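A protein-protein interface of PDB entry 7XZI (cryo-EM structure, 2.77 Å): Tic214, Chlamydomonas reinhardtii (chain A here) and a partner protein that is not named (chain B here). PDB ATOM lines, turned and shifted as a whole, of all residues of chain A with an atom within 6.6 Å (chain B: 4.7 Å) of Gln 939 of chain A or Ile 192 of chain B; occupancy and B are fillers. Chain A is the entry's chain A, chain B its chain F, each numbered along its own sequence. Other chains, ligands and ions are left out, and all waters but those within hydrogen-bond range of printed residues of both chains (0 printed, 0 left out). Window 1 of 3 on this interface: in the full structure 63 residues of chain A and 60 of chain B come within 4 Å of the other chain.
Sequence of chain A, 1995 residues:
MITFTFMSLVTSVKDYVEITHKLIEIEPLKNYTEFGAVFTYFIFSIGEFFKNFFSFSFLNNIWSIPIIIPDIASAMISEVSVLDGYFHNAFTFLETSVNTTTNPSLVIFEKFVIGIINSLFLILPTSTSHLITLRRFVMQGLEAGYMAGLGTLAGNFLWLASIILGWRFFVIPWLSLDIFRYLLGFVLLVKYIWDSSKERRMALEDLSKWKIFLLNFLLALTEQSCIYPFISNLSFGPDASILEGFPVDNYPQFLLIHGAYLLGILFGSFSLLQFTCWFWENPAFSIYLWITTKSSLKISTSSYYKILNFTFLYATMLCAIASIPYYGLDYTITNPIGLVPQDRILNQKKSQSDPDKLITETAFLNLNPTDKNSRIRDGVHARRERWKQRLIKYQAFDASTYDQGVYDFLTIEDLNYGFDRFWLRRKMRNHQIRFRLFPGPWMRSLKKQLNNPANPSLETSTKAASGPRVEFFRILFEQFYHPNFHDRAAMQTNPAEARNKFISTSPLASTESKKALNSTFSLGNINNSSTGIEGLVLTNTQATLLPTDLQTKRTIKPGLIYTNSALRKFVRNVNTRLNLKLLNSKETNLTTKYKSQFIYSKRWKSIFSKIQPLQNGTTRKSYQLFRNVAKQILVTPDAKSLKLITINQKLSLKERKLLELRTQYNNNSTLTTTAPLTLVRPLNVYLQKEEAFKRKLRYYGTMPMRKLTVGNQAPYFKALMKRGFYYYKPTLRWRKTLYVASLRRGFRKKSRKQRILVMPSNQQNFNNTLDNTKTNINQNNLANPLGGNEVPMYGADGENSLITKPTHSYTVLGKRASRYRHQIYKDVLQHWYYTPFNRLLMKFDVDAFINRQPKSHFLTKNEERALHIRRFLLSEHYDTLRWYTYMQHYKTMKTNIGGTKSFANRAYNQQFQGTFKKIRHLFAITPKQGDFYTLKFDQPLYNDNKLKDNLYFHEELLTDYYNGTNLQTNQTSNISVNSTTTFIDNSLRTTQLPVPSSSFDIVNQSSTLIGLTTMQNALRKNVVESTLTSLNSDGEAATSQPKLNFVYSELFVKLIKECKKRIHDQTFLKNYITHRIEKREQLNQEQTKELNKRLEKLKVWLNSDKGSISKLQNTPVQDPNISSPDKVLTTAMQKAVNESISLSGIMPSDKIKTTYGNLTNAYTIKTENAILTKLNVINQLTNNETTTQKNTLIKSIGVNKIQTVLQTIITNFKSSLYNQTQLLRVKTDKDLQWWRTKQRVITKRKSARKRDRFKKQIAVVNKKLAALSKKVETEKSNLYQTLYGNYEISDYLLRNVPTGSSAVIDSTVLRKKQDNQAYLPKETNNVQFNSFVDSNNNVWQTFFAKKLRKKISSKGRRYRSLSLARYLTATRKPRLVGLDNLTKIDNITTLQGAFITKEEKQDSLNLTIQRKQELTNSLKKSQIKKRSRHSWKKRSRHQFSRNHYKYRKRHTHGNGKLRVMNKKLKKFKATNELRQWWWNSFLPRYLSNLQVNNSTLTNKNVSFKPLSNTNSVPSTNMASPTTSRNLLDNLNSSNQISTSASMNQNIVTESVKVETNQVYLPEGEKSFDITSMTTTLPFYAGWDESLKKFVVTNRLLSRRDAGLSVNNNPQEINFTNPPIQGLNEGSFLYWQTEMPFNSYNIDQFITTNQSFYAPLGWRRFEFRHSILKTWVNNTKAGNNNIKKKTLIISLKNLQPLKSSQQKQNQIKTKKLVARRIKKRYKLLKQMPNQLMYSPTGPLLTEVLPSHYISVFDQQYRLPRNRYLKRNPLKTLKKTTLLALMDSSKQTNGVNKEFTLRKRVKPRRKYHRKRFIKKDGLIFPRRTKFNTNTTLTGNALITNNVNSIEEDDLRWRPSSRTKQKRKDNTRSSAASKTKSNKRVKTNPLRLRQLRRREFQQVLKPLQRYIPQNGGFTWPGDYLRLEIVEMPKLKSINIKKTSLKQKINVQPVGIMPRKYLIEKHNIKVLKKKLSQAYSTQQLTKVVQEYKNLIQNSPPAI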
ATOM      1  N   GLN A 853       2.419   2.178 -18.694  1.00  0.00           N
ATOM      2  CA  GLN A 853       1.520   1.189 -19.266  1.00  0.00           C
ATOM      3  C   GLN A 853       0.858   0.363 -18.163  1.00  0.00           C
ATOM      4  O   GLN A 853       1.384   0.264 -17.052  1.00  0.00           O
ATOM      5  CB  GLN A 853       2.277   0.271 -20.221  1.00  0.00           C
ATOM      6  CG  GLN A 853       3.280  -0.648 -19.553  1.00  0.00           C
ATOM      7  CD  GLN A 853       3.891  -1.634 -20.527  1.00  0.00           C
ATOM      8  OE1 GLN A 853       3.540  -1.657 -21.706  1.00  0.00           O
ATOM      9  NE2 GLN A 853       4.809  -2.457 -20.038  1.00  0.00           N
ATOM     10  N   HIS A 857       0.242  -5.781 -18.845  1.00  0.00           N
ATOM     11  CA  HIS A 857       0.871  -5.949 -20.148  1.00  0.00           C
ATOM     12  C   HIS A 857       2.279  -6.523 -20.061  1.00  0.00           C
ATOM     13  O   HIS A 857       2.882  -6.797 -21.105  1.00  0.00           O
ATOM     14  CB  HIS A 857       0.904  -4.614 -20.895  1.00  0.00           C
ATOM     15  CG  HIS A 857      -0.434  -4.169 -21.400  1.00  0.00           C
ATOM     16  ND1 HIS A 857      -0.581  -3.172 -22.340  1.00  0.00           N
ATOM     17  CD2 HIS A 857      -1.685  -4.588 -21.098  1.00  0.00           C
ATOM     18  CE1 HIS A 857      -1.865  -2.996 -22.596  1.00  0.00           C
ATOM     19  NE2 HIS A 857      -2.556  -3.843 -21.854  1.00  0.00           N
ATOM     20  N   PHE A 858       2.818  -6.708 -18.860  1.00  0.00           N
ATOM     21  CA  PHE A 858       4.122  -7.337 -18.704  1.00  0.00           C
ATOM     22  C   PHE A 858       3.981  -8.851 -18.806  1.00  0.00           C
ATOM     23  O   PHE A 858       3.042  -9.439 -18.265  1.00  0.00           O
ATOM     24  CB  PHE A 858       4.749  -6.954 -17.365  1.00  0.00           C
ATOM     25  CG  PHE A 858       5.140  -5.506 -17.266  1.00  0.00           C
ATOM     26  CD1 PHE A 858       4.196  -4.538 -16.970  1.00  0.00           C
ATOM     27  CD2 PHE A 858       6.455  -5.114 -17.459  1.00  0.00           C
ATOM     28  CE1 PHE A 858       4.552  -3.208 -16.875  1.00  0.00           C
ATOM     29  CE2 PHE A 858       6.818  -3.785 -17.365  1.00  0.00           C
ATOM     30  CZ  PHE A 858       5.865  -2.831 -17.071  1.00  0.00           C
ATOM     31  N   LEU A 859       4.921  -9.480 -19.508  1.00  0.00           N
ATOM     32  CA  LEU A 859       4.857 -10.908 -19.783  1.00  0.00           C
ATOM     33  C   LEU A 859       6.194 -11.568 -19.490  1.00  0.00           C
ATOM     34  O   LEU A 859       7.255 -10.955 -19.629  1.00  0.00           O
ATOM     35  CB  LEU A 859       4.466 -11.183 -21.241  1.00  0.00           C
ATOM     36  CG  LEU A 859       3.062 -10.775 -21.686  1.00  0.00           C
ATOM     37  CD1 LEU A 859       2.907 -10.976 -23.182  1.00  0.00           C
ATOM     38  CD2 LEU A 859       2.016 -11.571 -20.927  1.00  0.00           C
ATOM     39  N   GLU A 864       5.408 -15.440 -23.476  1.00  0.00           N
ATOM     40  CA  GLU A 864       5.556 -14.912 -24.830  1.00  0.00           C
ATOM     41  C   GLU A 864       5.745 -16.034 -25.847  1.00  0.00           C
ATOM     42  O   GLU A 864       5.140 -16.011 -26.928  1.00  0.00           O
ATOM     43  CB  GLU A 864       6.729 -13.934 -24.883  1.00  0.00           C
ATOM     44  CG  GLU A 864       6.935 -13.278 -26.238  1.00  0.00           C
ATOM     45  CD  GLU A 864       5.778 -12.383 -26.632  1.00  0.00           C
ATOM     46  OE1 GLU A 864       5.331 -11.579 -25.786  1.00  0.00           O
ATOM     47  OE2 GLU A 864       5.312 -12.488 -27.785  1.00  0.00           O
ATOM     48  N   LEU A 867       2.434 -17.706 -26.357  1.00  0.00           N
ATOM     49  CA  LEU A 867       1.571 -16.905 -27.220  1.00  0.00           C
ATOM     50  C   LEU A 867       1.973 -17.042 -28.684  1.00  0.00           C
ATOM     51  O   LEU A 867       1.109 -17.135 -29.563  1.00  0.00           O
ATOM     52  CB  LEU A 867       1.602 -15.438 -26.788  1.00  0.00           C
ATOM     53  CG  LEU A 867       0.974 -15.082 -25.438  1.00  0.00           C
ATOM     54  CD1 LEU A 867       1.054 -13.585 -25.178  1.00  0.00           C
ATOM     55  CD2 LEU A 867      -0.465 -15.563 -25.368  1.00  0.00           C
ATOM     56  N   LYS A 936      10.969  -7.310 -31.422  1.00  0.00           N
ATOM     57  CA  LYS A 936       9.864  -7.189 -32.360  1.00  0.00           C
ATOM     58  C   LYS A 936       9.012  -5.994 -31.965  1.00  0.00           C
ATOM     59  O   LYS A 936       9.078  -5.507 -30.835  1.00  0.00           O
ATOM     60  CB  LYS A 936       9.021  -8.469 -32.408  1.00  0.00           C
ATOM     61  CG  LYS A 936       8.526  -8.944 -31.054  1.00  0.00           C
ATOM     62  CD  LYS A 936       7.820 -10.282 -31.179  1.00  0.00           C
ATOM     63  CE  LYS A 936       7.339 -10.789 -29.832  1.00  0.00           C
ATOM     64  NZ  LYS A 936       6.680 -12.118 -29.956  1.00  0.00           N
ATOM     65  N   PHE A 937       8.208  -5.524 -32.917  1.00  0.00           N
ATOM     66  CA  PHE A 937       7.404  -4.323 -32.739  1.00  0.00           C
ATOM     67  C   PHE A 937       5.928  -4.627 -32.510  1.00  0.00           C
ATOM     68  O   PHE A 937       5.113  -3.699 -32.474  1.00  0.00           O
ATOM     69  CB  PHE A 937       7.569  -3.396 -33.945  1.00  0.00           C
ATOM     70  CG  PHE A 937       9.000  -3.069 -34.266  1.00  0.00           C
ATOM     71  CD1 PHE A 937       9.929  -2.882 -33.256  1.00  0.00           C
ATOM     72  CD2 PHE A 937       9.419  -2.959 -35.581  1.00  0.00           C
ATOM     73  CE1 PHE A 937      11.245  -2.584 -33.552  1.00  0.00           C
ATOM     74  CE2 PHE A 937      10.734  -2.662 -35.883  1.00  0.00           C
ATOM     75  CZ  PHE A 937      11.647  -2.475 -34.866  1.00  0.00           C
ATOM     76  N   ASP A 938       5.563  -5.895 -32.360  1.00  0.00           N
ATOM     77  CA  ASP A 938       4.200  -6.295 -32.053  1.00  0.00           C
ATOM     78  C   ASP A 938       4.161  -6.922 -30.665  1.00  0.00           C
ATOM     79  O   ASP A 938       5.195  -7.240 -30.072  1.00  0.00           O
ATOM     80  CB  ASP A 938       3.654  -7.272 -33.102  1.00  0.00           C
ATOM     81  CG  ASP A 938       4.470  -8.545 -33.194  1.00  0.00           C
ATOM     82  OD1 ASP A 938       5.688  -8.494 -32.929  1.00  0.00           O
ATOM     83  OD2 ASP A 938       3.893  -9.598 -33.535  1.00  0.00           O
ATOM     84  N   GLN A 939       2.953  -7.103 -30.147  1.00  0.00           N
ATOM     85  CA  GLN A 939       2.837  -7.557 -28.769  1.00  0.00           C
ATOM     86  C   GLN A 939       1.560  -8.355 -28.543  1.00  0.00           C
ATOM     87  O   GLN A 939       0.475  -7.772 -28.422  1.00  0.00           O
ATOM     88  CB  GLN A 939       2.887  -6.355 -27.825  1.00  0.00           C
ATOM     89  CG  GLN A 939       3.069  -6.710 -26.363  1.00  0.00           C
ATOM     90  CD  GLN A 939       3.166  -5.479 -25.484  1.00  0.00           C
ATOM     91  OE1 GLN A 939       2.561  -4.447 -25.771  1.00  0.00           O
ATOM     92  NE2 GLN A 939       3.940  -5.580 -24.410  1.00  0.00           N
ATOM     93  N   PRO A 940       1.643  -9.680 -28.492  1.00  0.00           N
ATOM     94  CA  PRO A 940       0.485 -10.480 -28.081  1.00  0.00           C
ATOM     95  C   PRO A 940       0.238 -10.354 -26.587  1.00  0.00           C
ATOM     96  O   PRO A 940       1.164 -10.196 -25.789  1.00  0.00           O
ATOM     97  CB  PRO A 940       0.892 -11.912 -28.457  1.00  0.00           C
ATOM     98  CG  PRO A 940       2.047 -11.760 -29.408  1.00  0.00           C
ATOM     99  CD  PRO A 940       2.748 -10.517 -28.981  1.00  0.00           C
ATOM    100  N   LEU A 941      -1.038 -10.424 -26.209  1.00  0.00           N
ATOM    101  CA  LEU A 941      -1.436 -10.210 -24.824  1.00  0.00           C
ATOM    102  C   LEU A 941      -2.519 -11.205 -24.427  1.00  0.00           C
ATOM    103  O   LEU A 941      -3.215 -11.769 -25.273  1.00  0.00           O
ATOM    104  CB  LEU A 941      -1.945  -8.780 -24.596  1.00  0.00           C
ATOM    105  CG  LEU A 941      -0.975  -7.626 -24.846  1.00  0.00           C
ATOM    106  CD1 LEU A 941      -1.682  -6.291 -24.690  1.00  0.00           C
ATOM    107  CD2 LEU A 941       0.211  -7.720 -23.904  1.00  0.00           C
ATOM    108  N   TRP B 145       1.575   8.322 -37.124  1.00  0.00           N
ATOM    109  CA  TRP B 145       0.656   7.205 -36.972  1.00  0.00           C
ATOM    110  C   TRP B 145      -0.641   7.465 -37.724  1.00  0.00           C
ATOM    111  O   TRP B 145      -1.005   8.609 -38.007  1.00  0.00           O
ATOM    112  CB  TRP B 145       0.353   6.947 -35.493  1.00  0.00           C
ATOM    113  CG  TRP B 145       1.580   6.769 -34.668  1.00  0.00           C
ATOM    114  CD1 TRP B 145       2.288   7.747 -34.035  1.00  0.00           C
ATOM    115  CD2 TRP B 145       2.258   5.539 -34.392  1.00  0.00           C
ATOM    116  NE1 TRP B 145       3.363   7.202 -33.377  1.00  0.00           N
ATOM    117  CE2 TRP B 145       3.367   5.848 -33.581  1.00  0.00           C
ATOM    118  CE3 TRP B 145       2.033   4.206 -34.750  1.00  0.00           C
ATOM    119  CZ2 TRP B 145       4.249   4.873 -33.121  1.00  0.00           C
ATOM    120  CZ3 TRP B 145       2.910   3.242 -34.294  1.00  0.00           C
ATOM    121  CH2 TRP B 145       4.005   3.579 -33.488  1.00  0.00           C
ATOM    122  N   PHE B 178      -4.340   0.795 -35.516  1.00  0.00           N
ATOM    123  CA  PHE B 178      -3.319   1.792 -35.797  1.00  0.00           C
ATOM    124  C   PHE B 178      -2.245   1.211 -36.708  1.00  0.00           C
ATOM    125  O   PHE B 178      -2.073  -0.006 -36.812  1.00  0.00           O
ATOM    126  CB  PHE B 178      -2.668   2.308 -34.505  1.00  0.00           C
ATOM    127  CG  PHE B 178      -3.406   3.446 -33.858  1.00  0.00           C
ATOM    128  CD1 PHE B 178      -4.430   3.204 -32.959  1.00  0.00           C
ATOM    129  CD2 PHE B 178      -3.063   4.759 -34.138  1.00  0.00           C
ATOM    130  CE1 PHE B 178      -5.105   4.249 -32.360  1.00  0.00           C
ATOM    131  CE2 PHE B 178      -3.734   5.808 -33.540  1.00  0.00           C
ATOM    132  CZ  PHE B 178      -4.756   5.551 -32.650  1.00  0.00           C
ATOM    133  N   LEU B 183       5.650  -1.361 -38.762  1.00  0.00           N
ATOM    134  CA  LEU B 183       4.737  -2.484 -38.905  1.00  0.00           C
ATOM    135  C   LEU B 183       4.471  -2.783 -40.375  1.00  0.00           C
ATOM    136  O   LEU B 183       4.816  -2.008 -41.272  1.00  0.00           O
ATOM    137  CB  LEU B 183       3.420  -2.201 -38.172  1.00  0.00           C
ATOM    138  CG  LEU B 183       3.560  -1.808 -36.701  1.00  0.00           C
ATOM    139  CD1 LEU B 183       2.206  -1.488 -36.093  1.00  0.00           C
ATOM    140  CD2 LEU B 183       4.260  -2.903 -35.911  1.00  0.00           C
ATOM    141  N   LEU B 187      -2.862  -3.075 -36.618  1.00  0.00           N
ATOM    142  CA  LEU B 187      -3.002  -3.819 -35.378  1.00  0.00           C
ATOM    143  C   LEU B 187      -3.732  -2.975 -34.346  1.00  0.00           C
ATOM    144  O   LEU B 187      -3.767  -1.744 -34.450  1.00  0.00           O
ATOM    145  CB  LEU B 187      -1.629  -4.234 -34.827  1.00  0.00           C
ATOM    146  CG  LEU B 187      -0.706  -5.012 -35.766  1.00  0.00           C
ATOM    147  CD1 LEU B 187       0.585  -5.386 -35.060  1.00  0.00           C
ATOM    148  CD2 LEU B 187      -1.404  -6.249 -36.303  1.00  0.00           C
ATOM    149  N   PRO B 188      -4.342  -3.610 -33.345  1.00  0.00           N
ATOM    150  CA  PRO B 188      -4.926  -2.845 -32.237  1.00  0.00           C
ATOM    151  C   PRO B 188      -3.862  -2.043 -31.504  1.00  0.00           C
ATOM    152  O   PRO B 188      -2.694  -2.429 -31.442  1.00  0.00           O
ATOM    153  CB  PRO B 188      -5.533  -3.929 -31.340  1.00  0.00           C
ATOM    154  CG  PRO B 188      -5.788  -5.074 -32.258  1.00  0.00           C
ATOM    155  CD  PRO B 188      -4.674  -5.043 -33.262  1.00  0.00           C
ATOM    156  N   ALA B 189      -4.288  -0.905 -30.948  1.00  0.00           N
ATOM    157  CA  ALA B 189      -3.345   0.029 -30.340  1.00  0.00           C
ATOM    158  C   ALA B 189      -2.581  -0.599 -29.183  1.00  0.00           C
ATOM    159  O   ALA B 189      -1.389  -0.322 -29.005  1.00  0.00           O
ATOM    160  CB  ALA B 189      -4.079   1.282 -29.866  1.00  0.00           C
ATOM    161  N   LYS B 190      -3.239  -1.439 -28.384  1.00  0.00           N
ATOM    162  CA  LYS B 190      -2.561  -2.060 -27.254  1.00  0.00           C
ATOM    163  C   LYS B 190      -1.614  -3.177 -27.671  1.00  0.00           C
ATOM    164  O   LYS B 190      -0.805  -3.616 -26.847  1.00  0.00           O
ATOM    165  CB  LYS B 190      -3.586  -2.598 -26.258  1.00  0.00           C
ATOM    166  CG  LYS B 190      -4.507  -3.656 -26.830  1.00  0.00           C
ATOM    167  CD  LYS B 190      -5.505  -4.118 -25.787  1.00  0.00           C
ATOM    168  CE  LYS B 190      -6.385  -5.232 -26.317  1.00  0.00           C
ATOM    169  NZ  LYS B 190      -7.338  -5.708 -25.280  1.00  0.00           N
ATOM    170  N   ASN B 191      -1.688  -3.645 -28.916  1.00  0.00           N
ATOM    171  CA  ASN B 191      -0.791  -4.683 -29.403  1.00  0.00           C
ATOM    172  C   ASN B 191       0.467  -4.127 -30.057  1.00  0.00           C
ATOM    173  O   ASN B 191       1.371  -4.904 -30.380  1.00  0.00           O
ATOM    174  CB  ASN B 191      -1.525  -5.600 -30.391  1.00  0.00           C
ATOM    175  CG  ASN B 191      -2.581  -6.459 -29.717  1.00  0.00           C
ATOM    176  OD1 ASN B 191      -3.752  -6.436 -30.093  1.00  0.00           O
ATOM    177  ND2 ASN B 191      -2.169  -7.223 -28.712  1.00  0.00           N
ATOM    178  N   ILE B 192       0.551  -2.814 -30.252  1.00  0.00           N
ATOM    179  CA  ILE B 192       1.792  -2.184 -30.688  1.00  0.00           C
ATOM    180  C   ILE B 192       2.708  -2.047 -29.480  1.00  0.00           C
ATOM    181  O   ILE B 192       2.246  -1.790 -28.361  1.00  0.00           O
ATOM    182  CB  ILE B 192       1.504  -0.827 -31.357  1.00  0.00           C
ATOM    183  CG1 ILE B 192       0.504  -1.008 -32.500  1.00  0.00           C
ATOM    184  CG2 ILE B 192       2.786  -0.194 -31.877  1.00  0.00           C
ATOM    185  CD1 ILE B 192       0.258   0.241 -33.319  1.00  0.00           C
ATOM    186  N   LYS B 193       4.011  -2.236 -29.701  1.00  0.00           N
ATOM    187  CA  LYS B 193       4.957  -2.403 -28.602  1.00  0.00           C
ATOM    188  C   LYS B 193       4.928  -1.220 -27.639  1.00  0.00           C
ATOM    189  O   LYS B 193       4.612  -1.371 -26.453  1.00  0.00           O
ATOM    190  CB  LYS B 193       6.366  -2.606 -29.159  1.00  0.00           C
ATOM    191  CG  LYS B 193       7.290  -3.362 -28.220  1.00  0.00           C
ATOM    192  CD  LYS B 193       6.681  -4.693 -27.826  1.00  0.00           C
ATOM    193  CE  LYS B 193       7.639  -5.523 -26.988  1.00  0.00           C
ATOM    194  NZ  LYS B 193       8.859  -5.905 -27.749  1.00  0.00           N
ATOM    195  N   LEU B 194       5.260  -0.028 -28.134  1.00  0.00           N
ATOM    196  CA  LEU B 194       5.333   1.176 -27.304  1.00  0.00           C
ATOM    197  C   LEU B 194       4.480   2.261 -27.949  1.00  0.00           C
ATOM    198  O   LEU B 194       4.994   3.114 -28.677  1.00  0.00           O
ATOM    199  CB  LEU B 194       6.778   1.634 -27.138  1.00  0.00           C
ATOM    200  CG  LEU B 194       7.763   0.612 -26.577  1.00  0.00           C
ATOM    201  CD1 LEU B 194       9.166   1.190 -26.548  1.00  0.00           C
ATOM    202  CD2 LEU B 194       7.331   0.180 -25.190  1.00  0.00           C
ATOM    203  N   LEU B 195       3.175   2.226 -27.687  1.00  0.00           N
ATOM    204  CA  LEU B 195       2.284   3.278 -28.158  1.00  0.00           C
ATOM    205  C   LEU B 195       1.443   3.826 -27.012  1.00  0.00           C
ATOM    206  O   LEU B 195       1.133   5.021 -26.976  1.00  0.00           O
ATOM    207  CB  LEU B 195       1.386   2.760 -29.280  1.00  0.00           C
ATOM    208  CG  LEU B 195       0.423   3.780 -29.880  1.00  0.00           C
ATOM    209  CD1 LEU B 195       1.181   5.000 -30.383  1.00  0.00           C
ATOM    210  CD2 LEU B 195      -0.377   3.144 -30.998  1.00  0.00           C
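ND2 of Asn 191 of chain B is in hydrogen-bond range of O of Gln 939 of chain A, 2.7 Å away.
The backbone NH (N) of Lys 193 of chain B sits at hydrogen-bond distance from the backbone carbonyl oxygen (O) of Phe 937 of chain A (3.3 Å).
NZ of Lys 193 of chain B is in hydrogen-bond range of O of Lys 936 of chain A, 3.1 Å away.
NZ of Lys 936 of chain A lies within salt-bridge range of OE2 of Glu 864 of chain A (2.6 Å).
Phe 937 of chain A touches Leu 183 of chain B (O to CD2, 3.6 Å).
C of Asp 938 of chain A touches O of Asn 191 of chain B, at 3.5 Å.
Lys 193 of chain B touches Asp 938 of chain A.
Lys 190 of chain B touches Gln 939 of chain A.
Ile 192 of chain B touches Gln 939 of chain A (O to OE1, 3.7 Å).
Gln 939 of chain A touches Lys 193 of chain B.
CD1 of Leu 941 of chain A touches O of Lys 190 of chain B, 3.5 Å away.
Of chain B, only Lys 190, Asn 191, Ile 192 and Lys 193 come within 4 Å of Gln 939 of chain A.
Of the printed residues of chain A, Ile 192 of chain B touches Gln 939 (3.7 Å).
Of the printed residues of chain B, Phe 937 of chain A touches Leu 183 and Lys 193.
Of the printed residues of chain A, Lys 193 of chain B touches Lys 936 (3.1 Å), Phe 937 (3.3 Å), Asp 938 (3.7 Å) and Gln 939 (3.8 Å).
Printed residues of chain B within 4 Å of Asp 938 of chain A: Asn 191 and Lys 193.
Printed residues of chain B within 4 Å of Lys 936 of chain A: Lys 193.
Gln 853 of chain A touches none of the printed residues of chain B.
The nearest printed residue of chain B that does not touch Gln 939 of chain A is Leu 194 of chain B (5.7 Å).
Printed residues of chain A that touch a printed residue of chain B: Lys 936, Phe 937, Asp 938, Gln 939 and Leu 941.
Hydrophobic or aromatic side chains of chain A that line the printed part of chain B: Phe 937 and Leu 941.
Of the 12 printed residues of chain B, 5 touch a printed residue of chain A.
Hydrophobic or aromatic side chains of chain B that line the printed part of chain A: Leu 183.
Among the printed residues, no Asp or Glu carboxylate lies within 4 Å of a Lys or Arg side-chain nitrogen of the other chain.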
